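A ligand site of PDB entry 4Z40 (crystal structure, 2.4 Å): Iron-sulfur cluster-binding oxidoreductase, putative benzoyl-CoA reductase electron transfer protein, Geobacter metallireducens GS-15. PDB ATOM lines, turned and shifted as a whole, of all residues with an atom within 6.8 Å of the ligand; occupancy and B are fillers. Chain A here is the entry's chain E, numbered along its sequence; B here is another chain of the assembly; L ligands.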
ATOM      1  N   ILE A  15       3.506 -32.694  24.241  1.00  0.00           N
ATOM      2  CA  ILE A  15       3.863 -32.107  22.984  1.00  0.00           C
ATOM      3  C   ILE A  15       5.197 -32.655  22.511  1.00  0.00           C
ATOM      4  O   ILE A  15       6.216 -32.459  23.165  1.00  0.00           O
ATOM      5  CB  ILE A  15       3.916 -30.569  23.095  1.00  0.00           C
ATOM      6  CG1 ILE A  15       2.548 -30.044  23.566  1.00  0.00           C
ATOM      7  CG2 ILE A  15       4.318 -29.921  21.775  1.00  0.00           C
ATOM      8  CD1 ILE A  15       2.491 -28.544  23.717  1.00  0.00           C
ATOM      9  N   ASP A  16       5.176 -33.352  21.367  1.00  0.00           N
ATOM     10  CA  ASP A  16       6.403 -33.827  20.755  1.00  0.00           C
ATOM     11  C   ASP A  16       6.798 -32.864  19.657  1.00  0.00           C
ATOM     12  O   ASP A  16       6.514 -33.081  18.470  1.00  0.00           O
ATOM     13  CB  ASP A  16       6.229 -35.255  20.211  1.00  0.00           C
ATOM     14  CG  ASP A  16       7.573 -35.924  19.904  1.00  0.00           C
ATOM     15  OD1 ASP A  16       8.571 -35.207  19.685  1.00  0.00           O
ATOM     16  OD2 ASP A  16       7.621 -37.182  19.860  1.00  0.00           O
ATOM     17  N   LYS A  19       8.123 -33.966  16.373  1.00  0.00           N
ATOM     18  CA  LYS A  19       7.219 -34.497  15.367  1.00  0.00           C
ATOM     19  C   LYS A  19       6.491 -33.401  14.602  1.00  0.00           C
ATOM     20  O   LYS A  19       5.992 -33.641  13.491  1.00  0.00           O
ATOM     21  CB  LYS A  19       6.195 -35.436  15.993  1.00  0.00           C
ATOM     22  CG  LYS A  19       6.710 -36.794  16.419  1.00  0.00           C
ATOM     23  CD  LYS A  19       5.645 -37.532  17.211  1.00  0.00           C
ATOM     24  CE  LYS A  19       5.676 -39.022  16.952  1.00  0.00           C
ATOM     25  NZ  LYS A  19       4.472 -39.718  17.497  1.00  0.00           N
ATOM     26  N   CYS A  20       6.425 -32.207  15.191  1.00  0.00           N
ATOM     27  CA  CYS A  20       5.634 -31.134  14.590  1.00  0.00           C
ATOM     28  C   CYS A  20       6.169 -30.734  13.224  1.00  0.00           C
ATOM     29  O   CYS A  20       7.375 -30.637  13.019  1.00  0.00           O
ATOM     30  CB  CYS A  20       5.602 -29.912  15.497  1.00  0.00           C
ATOM     31  SG  CYS A  20       4.596 -28.571  14.848  1.00  0.00           S
ATOM     32  N   ASN A  21       5.273 -30.491  12.277  1.00  0.00           N
ATOM     33  CA  ASN A  21       5.716 -30.023  10.966  1.00  0.00           C
ATOM     34  C   ASN A  21       5.360 -28.555  10.717  1.00  0.00           C
ATOM     35  O   ASN A  21       5.698 -28.012   9.669  1.00  0.00           O
ATOM     36  CB  ASN A  21       5.156 -30.907   9.854  1.00  0.00           C
ATOM     37  CG  ASN A  21       3.669 -31.187  10.002  1.00  0.00           C
ATOM     38  OD1 ASN A  21       2.846 -30.282   9.880  1.00  0.00           O
ATOM     39  ND2 ASN A  21       3.339 -32.437  10.237  1.00  0.00           N
ATOM     40  N   GLY A  22       4.703 -27.923  11.689  1.00  0.00           N
ATOM     41  CA  GLY A  22       4.434 -26.500  11.624  1.00  0.00           C
ATOM     42  C   GLY A  22       3.261 -26.126  10.727  1.00  0.00           C
ATOM     43  O   GLY A  22       3.107 -24.956  10.367  1.00  0.00           O
ATOM     44  N   CYS A  23       2.446 -27.112  10.384  1.00  0.00           N
ATOM     45  CA  CYS A  23       1.292 -26.907   9.503  1.00  0.00           C
ATOM     46  C   CYS A  23       0.275 -25.904  10.068  1.00  0.00           C
ATOM     47  O   CYS A  23      -0.495 -25.307   9.310  1.00  0.00           O
ATOM     48  CB  CYS A  23       0.596 -28.243   9.227  1.00  0.00           C
ATOM     49  SG  CYS A  23      -0.334 -28.887  10.616  1.00  0.00           S
ATOM     50  N   ARG A  24       0.283 -25.754  11.393  1.00  0.00           N
ATOM     51  CA  ARG A  24      -0.592 -24.822  12.102  1.00  0.00           C
ATOM     52  C   ARG A  24      -2.079 -25.195  12.016  1.00  0.00           C
ATOM     53  O   ARG A  24      -2.951 -24.336  12.213  1.00  0.00           O
ATOM     54  CB  ARG A  24      -0.362 -23.391  11.593  1.00  0.00           C
ATOM     55  CG  ARG A  24       1.044 -22.848  11.896  1.00  0.00           C
ATOM     56  CD  ARG A  24       1.254 -21.409  11.437  1.00  0.00           C
ATOM     57  NE  ARG A  24       0.080 -20.581  11.687  1.00  0.00           N
ATOM     58  CZ  ARG A  24      -0.321 -19.592  10.887  1.00  0.00           C
ATOM     59  NH1 ARG A  24       0.376 -19.300   9.786  1.00  0.00           N
ATOM     60  NH2 ARG A  24      -1.425 -18.894  11.194  1.00  0.00           N
ATOM     61  N   ALA A  25      -2.372 -26.472  11.764  1.00  0.00           N
ATOM     62  CA  ALA A  25      -3.750 -26.964  11.674  1.00  0.00           C
ATOM     63  C   ALA A  25      -4.482 -26.898  13.019  1.00  0.00           C
ATOM     64  O   ALA A  25      -5.665 -26.544  13.069  1.00  0.00           O
ATOM     65  CB  ALA A  25      -3.773 -28.401  11.162  1.00  0.00           C
ATOM     66  N   CYS A  26      -3.776 -27.268  14.084  1.00  0.00           N
ATOM     67  CA  CYS A  26      -4.291 -27.088  15.450  1.00  0.00           C
ATOM     68  C   CYS A  26      -4.853 -25.688  15.652  1.00  0.00           C
ATOM     69  O   CYS A  26      -5.969 -25.532  16.167  1.00  0.00           O
ATOM     70  CB  CYS A  26      -3.166 -27.351  16.465  1.00  0.00           C
ATOM     71  SG  CYS A  26      -1.592 -26.739  15.893  1.00  0.00           S
ATOM     72  N   GLU A  27      -4.092 -24.684  15.210  1.00  0.00           N
ATOM     73  CA  GLU A  27      -4.508 -23.281  15.341  1.00  0.00           C
ATOM     74  C   GLU A  27      -5.833 -23.029  14.638  1.00  0.00           C
ATOM     75  O   GLU A  27      -6.702 -22.326  15.152  1.00  0.00           O
ATOM     76  CB  GLU A  27      -3.439 -22.328  14.782  1.00  0.00           C
ATOM     77  CG  GLU A  27      -2.156 -22.205  15.598  1.00  0.00           C
ATOM     78  CD  GLU A  27      -1.302 -21.031  15.122  1.00  0.00           C
ATOM     79  OE1 GLU A  27      -1.742 -20.342  14.191  1.00  0.00           O
ATOM     80  OE2 GLU A  27      -0.203 -20.789  15.678  1.00  0.00           O
ATOM     81  N   VAL A  49      -4.123 -22.480  21.108  1.00  0.00           N
ATOM     82  CA  VAL A  49      -2.842 -23.103  20.845  1.00  0.00           C
ATOM     83  C   VAL A  49      -2.188 -22.342  19.704  1.00  0.00           C
ATOM     84  O   VAL A  49      -2.818 -22.082  18.686  1.00  0.00           O
ATOM     85  CB  VAL A  49      -2.984 -24.604  20.508  1.00  0.00           C
ATOM     86  CG1 VAL A  49      -4.002 -24.828  19.363  1.00  0.00           C
ATOM     87  CG2 VAL A  49      -1.642 -25.217  20.176  1.00  0.00           C
ATOM     88  N   VAL A  51       1.539 -21.967  17.464  1.00  0.00           N
ATOM     89  CA  VAL A  51       2.813 -22.604  17.183  1.00  0.00           C
ATOM     90  C   VAL A  51       3.949 -21.584  17.091  1.00  0.00           C
ATOM     91  O   VAL A  51       3.870 -20.624  16.349  1.00  0.00           O
ATOM     92  CB  VAL A  51       2.732 -23.403  15.886  1.00  0.00           C
ATOM     93  CG1 VAL A  51       4.050 -24.098  15.614  1.00  0.00           C
ATOM     94  CG2 VAL A  51       1.588 -24.415  15.970  1.00  0.00           C
ATOM     95  N   TYR A  60       9.948 -25.541  16.033  1.00  0.00           N
ATOM     96  CA  TYR A  60       8.504 -25.762  15.881  1.00  0.00           C
ATOM     97  C   TYR A  60       7.984 -26.197  17.224  1.00  0.00           C
ATOM     98  O   TYR A  60       8.210 -27.332  17.648  1.00  0.00           O
ATOM     99  CB  TYR A  60       8.193 -26.831  14.823  1.00  0.00           C
ATOM    100  CG  TYR A  60       8.845 -26.575  13.479  1.00  0.00           C
ATOM    101  CD1 TYR A  60      10.157 -26.967  13.251  1.00  0.00           C
ATOM    102  CD2 TYR A  60       8.141 -25.954  12.448  1.00  0.00           C
ATOM    103  CE1 TYR A  60      10.751 -26.730  12.035  1.00  0.00           C
ATOM    104  CE2 TYR A  60       8.722 -25.715  11.246  1.00  0.00           C
ATOM    105  CZ  TYR A  60      10.034 -26.114  11.035  1.00  0.00           C
ATOM    106  OH  TYR A  60      10.636 -25.898   9.815  1.00  0.00           O
ATOM    107  N   PRO A  62       4.534 -25.907  19.598  1.00  0.00           N
ATOM    108  CA  PRO A  62       3.147 -25.642  19.980  1.00  0.00           C
ATOM    109  C   PRO A  62       3.029 -25.121  21.407  1.00  0.00           C
ATOM    110  O   PRO A  62       3.434 -25.810  22.346  1.00  0.00           O
ATOM    111  CB  PRO A  62       2.494 -27.019  19.861  1.00  0.00           C
ATOM    112  CG  PRO A  62       3.332 -27.766  18.896  1.00  0.00           C
ATOM    113  CD  PRO A  62       4.730 -27.287  19.132  1.00  0.00           C
ATOM    114  N   TYR A  64       0.414 -23.628  24.414  1.00  0.00           N
ATOM    115  CA  TYR A  64      -0.971 -23.566  24.856  1.00  0.00           C
ATOM    116  C   TYR A  64      -1.236 -22.359  25.780  1.00  0.00           C
ATOM    117  O   TYR A  64      -0.373 -21.943  26.557  1.00  0.00           O
ATOM    118  CB  TYR A  64      -1.352 -24.875  25.563  1.00  0.00           C
ATOM    119  CG  TYR A  64      -1.672 -25.997  24.601  1.00  0.00           C
ATOM    120  CD1 TYR A  64      -0.654 -26.757  24.028  1.00  0.00           C
ATOM    121  CD2 TYR A  64      -2.981 -26.292  24.242  1.00  0.00           C
ATOM    122  CE1 TYR A  64      -0.939 -27.764  23.136  1.00  0.00           C
ATOM    123  CE2 TYR A  64      -3.280 -27.299  23.351  1.00  0.00           C
ATOM    124  CZ  TYR A  64      -2.248 -28.034  22.802  1.00  0.00           C
ATOM    125  OH  TYR A  64      -2.526 -29.052  21.905  1.00  0.00           O
ATOM    126  N   CYS A 124      -7.595 -29.910  18.743  1.00  0.00           N
ATOM    127  CA  CYS A 124      -6.210 -29.693  18.329  1.00  0.00           C
ATOM    128  C   CYS A 124      -5.543 -31.049  18.122  1.00  0.00           C
ATOM    129  O   CYS A 124      -4.870 -31.282  17.105  1.00  0.00           O
ATOM    130  CB  CYS A 124      -5.420 -28.838  19.345  1.00  0.00           C
ATOM    131  SG  CYS A 124      -5.510 -29.276  21.148  1.00  0.00           S
ATOM    132  N   TRP A 127      -6.903 -33.137  14.972  1.00  0.00           N
ATOM    133  CA  TRP A 127      -6.553 -32.653  13.655  1.00  0.00           C
ATOM    134  C   TRP A 127      -5.054 -32.707  13.402  1.00  0.00           C
ATOM    135  O   TRP A 127      -4.592 -32.415  12.289  1.00  0.00           O
ATOM    136  CB  TRP A 127      -7.069 -31.223  13.454  1.00  0.00           C
ATOM    137  CG  TRP A 127      -8.469 -31.204  12.991  1.00  0.00           C
ATOM    138  CD1 TRP A 127      -9.498 -31.971  13.449  1.00  0.00           C
ATOM    139  CD2 TRP A 127      -9.010 -30.411  11.922  1.00  0.00           C
ATOM    140  NE1 TRP A 127     -10.646 -31.690  12.756  1.00  0.00           N
ATOM    141  CE2 TRP A 127     -10.371 -30.745  11.809  1.00  0.00           C
ATOM    142  CE3 TRP A 127      -8.470 -29.452  11.057  1.00  0.00           C
ATOM    143  CZ2 TRP A 127     -11.206 -30.143  10.866  1.00  0.00           C
ATOM    144  CZ3 TRP A 127      -9.297 -28.858  10.122  1.00  0.00           C
ATOM    145  CH2 TRP A 127     -10.650 -29.207  10.034  1.00  0.00           C
ATOM    146  N   CYS A 128      -4.294 -33.064  14.419  1.00  0.00           N
ATOM    147  CA  CYS A 128      -2.853 -33.219  14.237  1.00  0.00           C
ATOM    148  C   CYS A 128      -2.555 -34.650  13.806  1.00  0.00           C
ATOM    149  O   CYS A 128      -2.221 -35.504  14.634  1.00  0.00           O
ATOM    150  CB  CYS A 128      -2.102 -32.865  15.526  1.00  0.00           C
ATOM    151  SG  CYS A 128      -0.329 -32.965  15.358  1.00  0.00           S
ATOM    152  N   LEU A 129      -2.672 -34.912  12.505  1.00  0.00           N
ATOM    153  CA  LEU A 129      -2.599 -36.267  11.975  1.00  0.00           C
ATOM    154  C   LEU A 129      -1.236 -36.941  12.143  1.00  0.00           C
ATOM    155  O   LEU A 129      -1.156 -38.167  12.207  1.00  0.00           O
ATOM    156  CB  LEU A 129      -3.014 -36.287  10.497  1.00  0.00           C
ATOM    157  CG  LEU A 129      -4.445 -36.708  10.195  1.00  0.00           C
ATOM    158  CD1 LEU A 129      -5.435 -35.690  10.727  1.00  0.00           C
ATOM    159  CD2 LEU A 129      -4.670 -36.949   8.693  1.00  0.00           C
ATOM    160  N   VAL A 130      -0.164 -36.166  12.221  1.00  0.00           N
ATOM    161  CA  VAL A 130       1.159 -36.730  12.500  1.00  0.00           C
ATOM    162  C   VAL A 130       1.281 -37.160  13.963  1.00  0.00           C
ATOM    163  O   VAL A 130       2.195 -37.903  14.340  1.00  0.00           O
ATOM    164  CB  VAL A 130       2.285 -35.716  12.150  1.00  0.00           C
ATOM    165  CG1 VAL A 130       2.300 -34.549  13.137  1.00  0.00           C
ATOM    166  CG2 VAL A 130       3.654 -36.408  12.106  1.00  0.00           C
ATOM    167  N   GLY A 131       0.362 -36.702  14.811  1.00  0.00           N
ATOM    168  CA  GLY A 131       0.289 -37.133  16.202  1.00  0.00           C
ATOM    169  C   GLY A 131       1.289 -36.516  17.160  1.00  0.00           C
ATOM    170  O   GLY A 131       1.867 -37.216  18.002  1.00  0.00           O
ATOM    171  N   ALA A 132       1.483 -35.211  17.079  1.00  0.00           N
ATOM    172  CA  ALA A 132       2.455 -34.533  17.934  1.00  0.00           C
ATOM    173  C   ALA A 132       1.813 -34.148  19.275  1.00  0.00           C
ATOM    174  O   ALA A 132       2.505 -33.720  20.207  1.00  0.00           O
ATOM    175  CB  ALA A 132       3.014 -33.299  17.227  1.00  0.00           C
ATOM    176  N   LEU A 133       0.497 -34.312  19.360  1.00  0.00           N
ATOM    177  CA  LEU A 133      -0.270 -33.838  20.487  1.00  0.00           C
ATOM    178  C   LEU A 133      -1.106 -34.944  21.109  1.00  0.00           C
ATOM    179  O   LEU A 133      -1.794 -35.679  20.391  1.00  0.00           O
ATOM    180  CB  LEU A 133      -1.197 -32.697  20.066  1.00  0.00           C
ATOM    181  CG  LEU A 133      -0.611 -31.530  19.270  1.00  0.00           C
ATOM    182  CD1 LEU A 133      -1.729 -30.541  18.941  1.00  0.00           C
ATOM    183  CD2 LEU A 133       0.506 -30.829  20.050  1.00  0.00           C
ATOM    184  N   SER B 298       5.288 -28.956   6.469  1.00  0.00           N
ATOM    185  CA  SER B 298       4.069 -28.797   5.686  1.00  0.00           C
ATOM    186  C   SER B 298       3.736 -27.369   5.270  1.00  0.00           C
ATOM    187  O   SER B 298       4.174 -26.393   5.909  1.00  0.00           O
ATOM    188  CB  SER B 298       2.892 -29.332   6.495  1.00  0.00           C
ATOM    189  OG  SER B 298       2.961 -30.726   6.699  1.00  0.00           O
ATOM    190  N   CYS B 302      -1.963 -28.677   6.457  1.00  0.00           N
ATOM    191  CA  CYS B 302      -1.781 -29.930   5.738  1.00  0.00           C
ATOM    192  C   CYS B 302      -0.846 -30.892   6.471  1.00  0.00           C
ATOM    193  O   CYS B 302       0.204 -30.492   6.957  1.00  0.00           O
ATOM    194  CB  CYS B 302      -1.237 -29.669   4.333  1.00  0.00           C
ATOM    195  SG  CYS B 302      -1.220 -31.139   3.242  1.00  0.00           S
ATOM    196  N   PRO B 303      -1.218 -32.176   6.533  1.00  0.00           N
ATOM    197  CA  PRO B 303      -0.369 -33.138   7.226  1.00  0.00           C
ATOM    198  C   PRO B 303       0.661 -33.843   6.340  1.00  0.00           C
ATOM    199  O   PRO B 303       1.413 -34.659   6.851  1.00  0.00           O
ATOM    200  CB  PRO B 303      -1.389 -34.148   7.743  1.00  0.00           C
ATOM    201  CG  PRO B 303      -2.431 -34.165   6.683  1.00  0.00           C
ATOM    202  CD  PRO B 303      -2.513 -32.748   6.160  1.00  0.00           C
HETATM  203 FE1  LIG L   1      -0.037 -28.228  15.175  1.00  0.00          FE
HETATM  204 FE2  LIG L   1       0.358 -30.914  14.705  1.00  0.00          FE
HETATM  205 FE3  LIG L   1       2.399 -29.146  14.910  1.00  0.00          FE
HETATM  206 FE4  LIG L   1       0.660 -29.248  12.683  1.00  0.00          FE
HETATM  207  S1  LIG L   1       2.196 -30.816  13.325  1.00  0.00           S
HETATM  208  S2  LIG L   1       1.538 -27.372  13.767  1.00  0.00           S
HETATM  209  S3  LIG L   1      -1.308 -29.610  13.813  1.00  0.00           S
HETATM  210  S4  LIG L   1       0.962 -29.726  16.587  1.00  0.00           S
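N of Ala 132 sits close to SG of Cys 128 (3.4 Å).
The side-chain sulfur (SG) of Cys 20 lies close to the backbone NH (N) of Gly 22 (3.2 Å).
The backbone NH (N) of Cys 23 sits close to the side-chain amide oxygen (OD1) of Asn 21 (3.2 Å).
The side-chain sulfur (SG) of Cys 23 lies close to the backbone NH (N) of Ala 25, at 3.4 Å.
OE1 of Glu 27 is in salt-bridge range of NE of Arg 24, 3.1 Å away.
OD1 of Asn 21 is in hydrogen-bond range of OG of Ser 298 of chain B, at 3.2 Å.
The backbone NH of Val 51 sits at hydrogen-bond distance from the side-chain carboxylate of Glu 27, at 2.8 Å.
The side-chain sulfur of Cys 128 is bound to an iron atom (FE2) of the ligand.
N of Cys 26 sits close to S3 of the ligand (3.4 Å).
The side-chain sulfur of Cys 26 binds an iron atom (FE1) of the ligand, at 2.3 Å.
The side-chain sulfur (SG) of Cys 20 is bound to an iron atom (FE3) of the ligand (2.3 Å).
A sulfur (S2) of the ligand lies close to the backbone NH (N) of Cys 23, at 3.5 Å.
SG of Cys 23 binds FE4 of the ligand (2.3 Å).
A sulfur (S2) of the ligand sits close to the backbone NH (N) of Arg 24.
The backbone NH (N) of Asn 21 lies close to a sulfur (S1) of the ligand, at 3.3 Å.
The side-chain amide oxygen (OD1) of Asn 21 lies close to a sulfur (S1) of the ligand (3.5 Å).
Merely in contact with the ligand: Leu 133 (3.6 Å), Val 51 (3.7 Å), Gly 22 (3.7 Å), Val 130 (3.7 Å), Ala 25 (3.8 Å) and Pro 62 (3.8 Å).
Hydrophobic or aromatic side chains that line the ligand: Ala 25, Val 51, Pro 62, Val 130 and Leu 133.
Within 4 Å of the ligand: Cys 20, Asn 21, Gly 22, Cys 23, Arg 24, Ala 25, Cys 26, Val 51, Pro 62, Cys 128, Val 130 and Leu 133.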
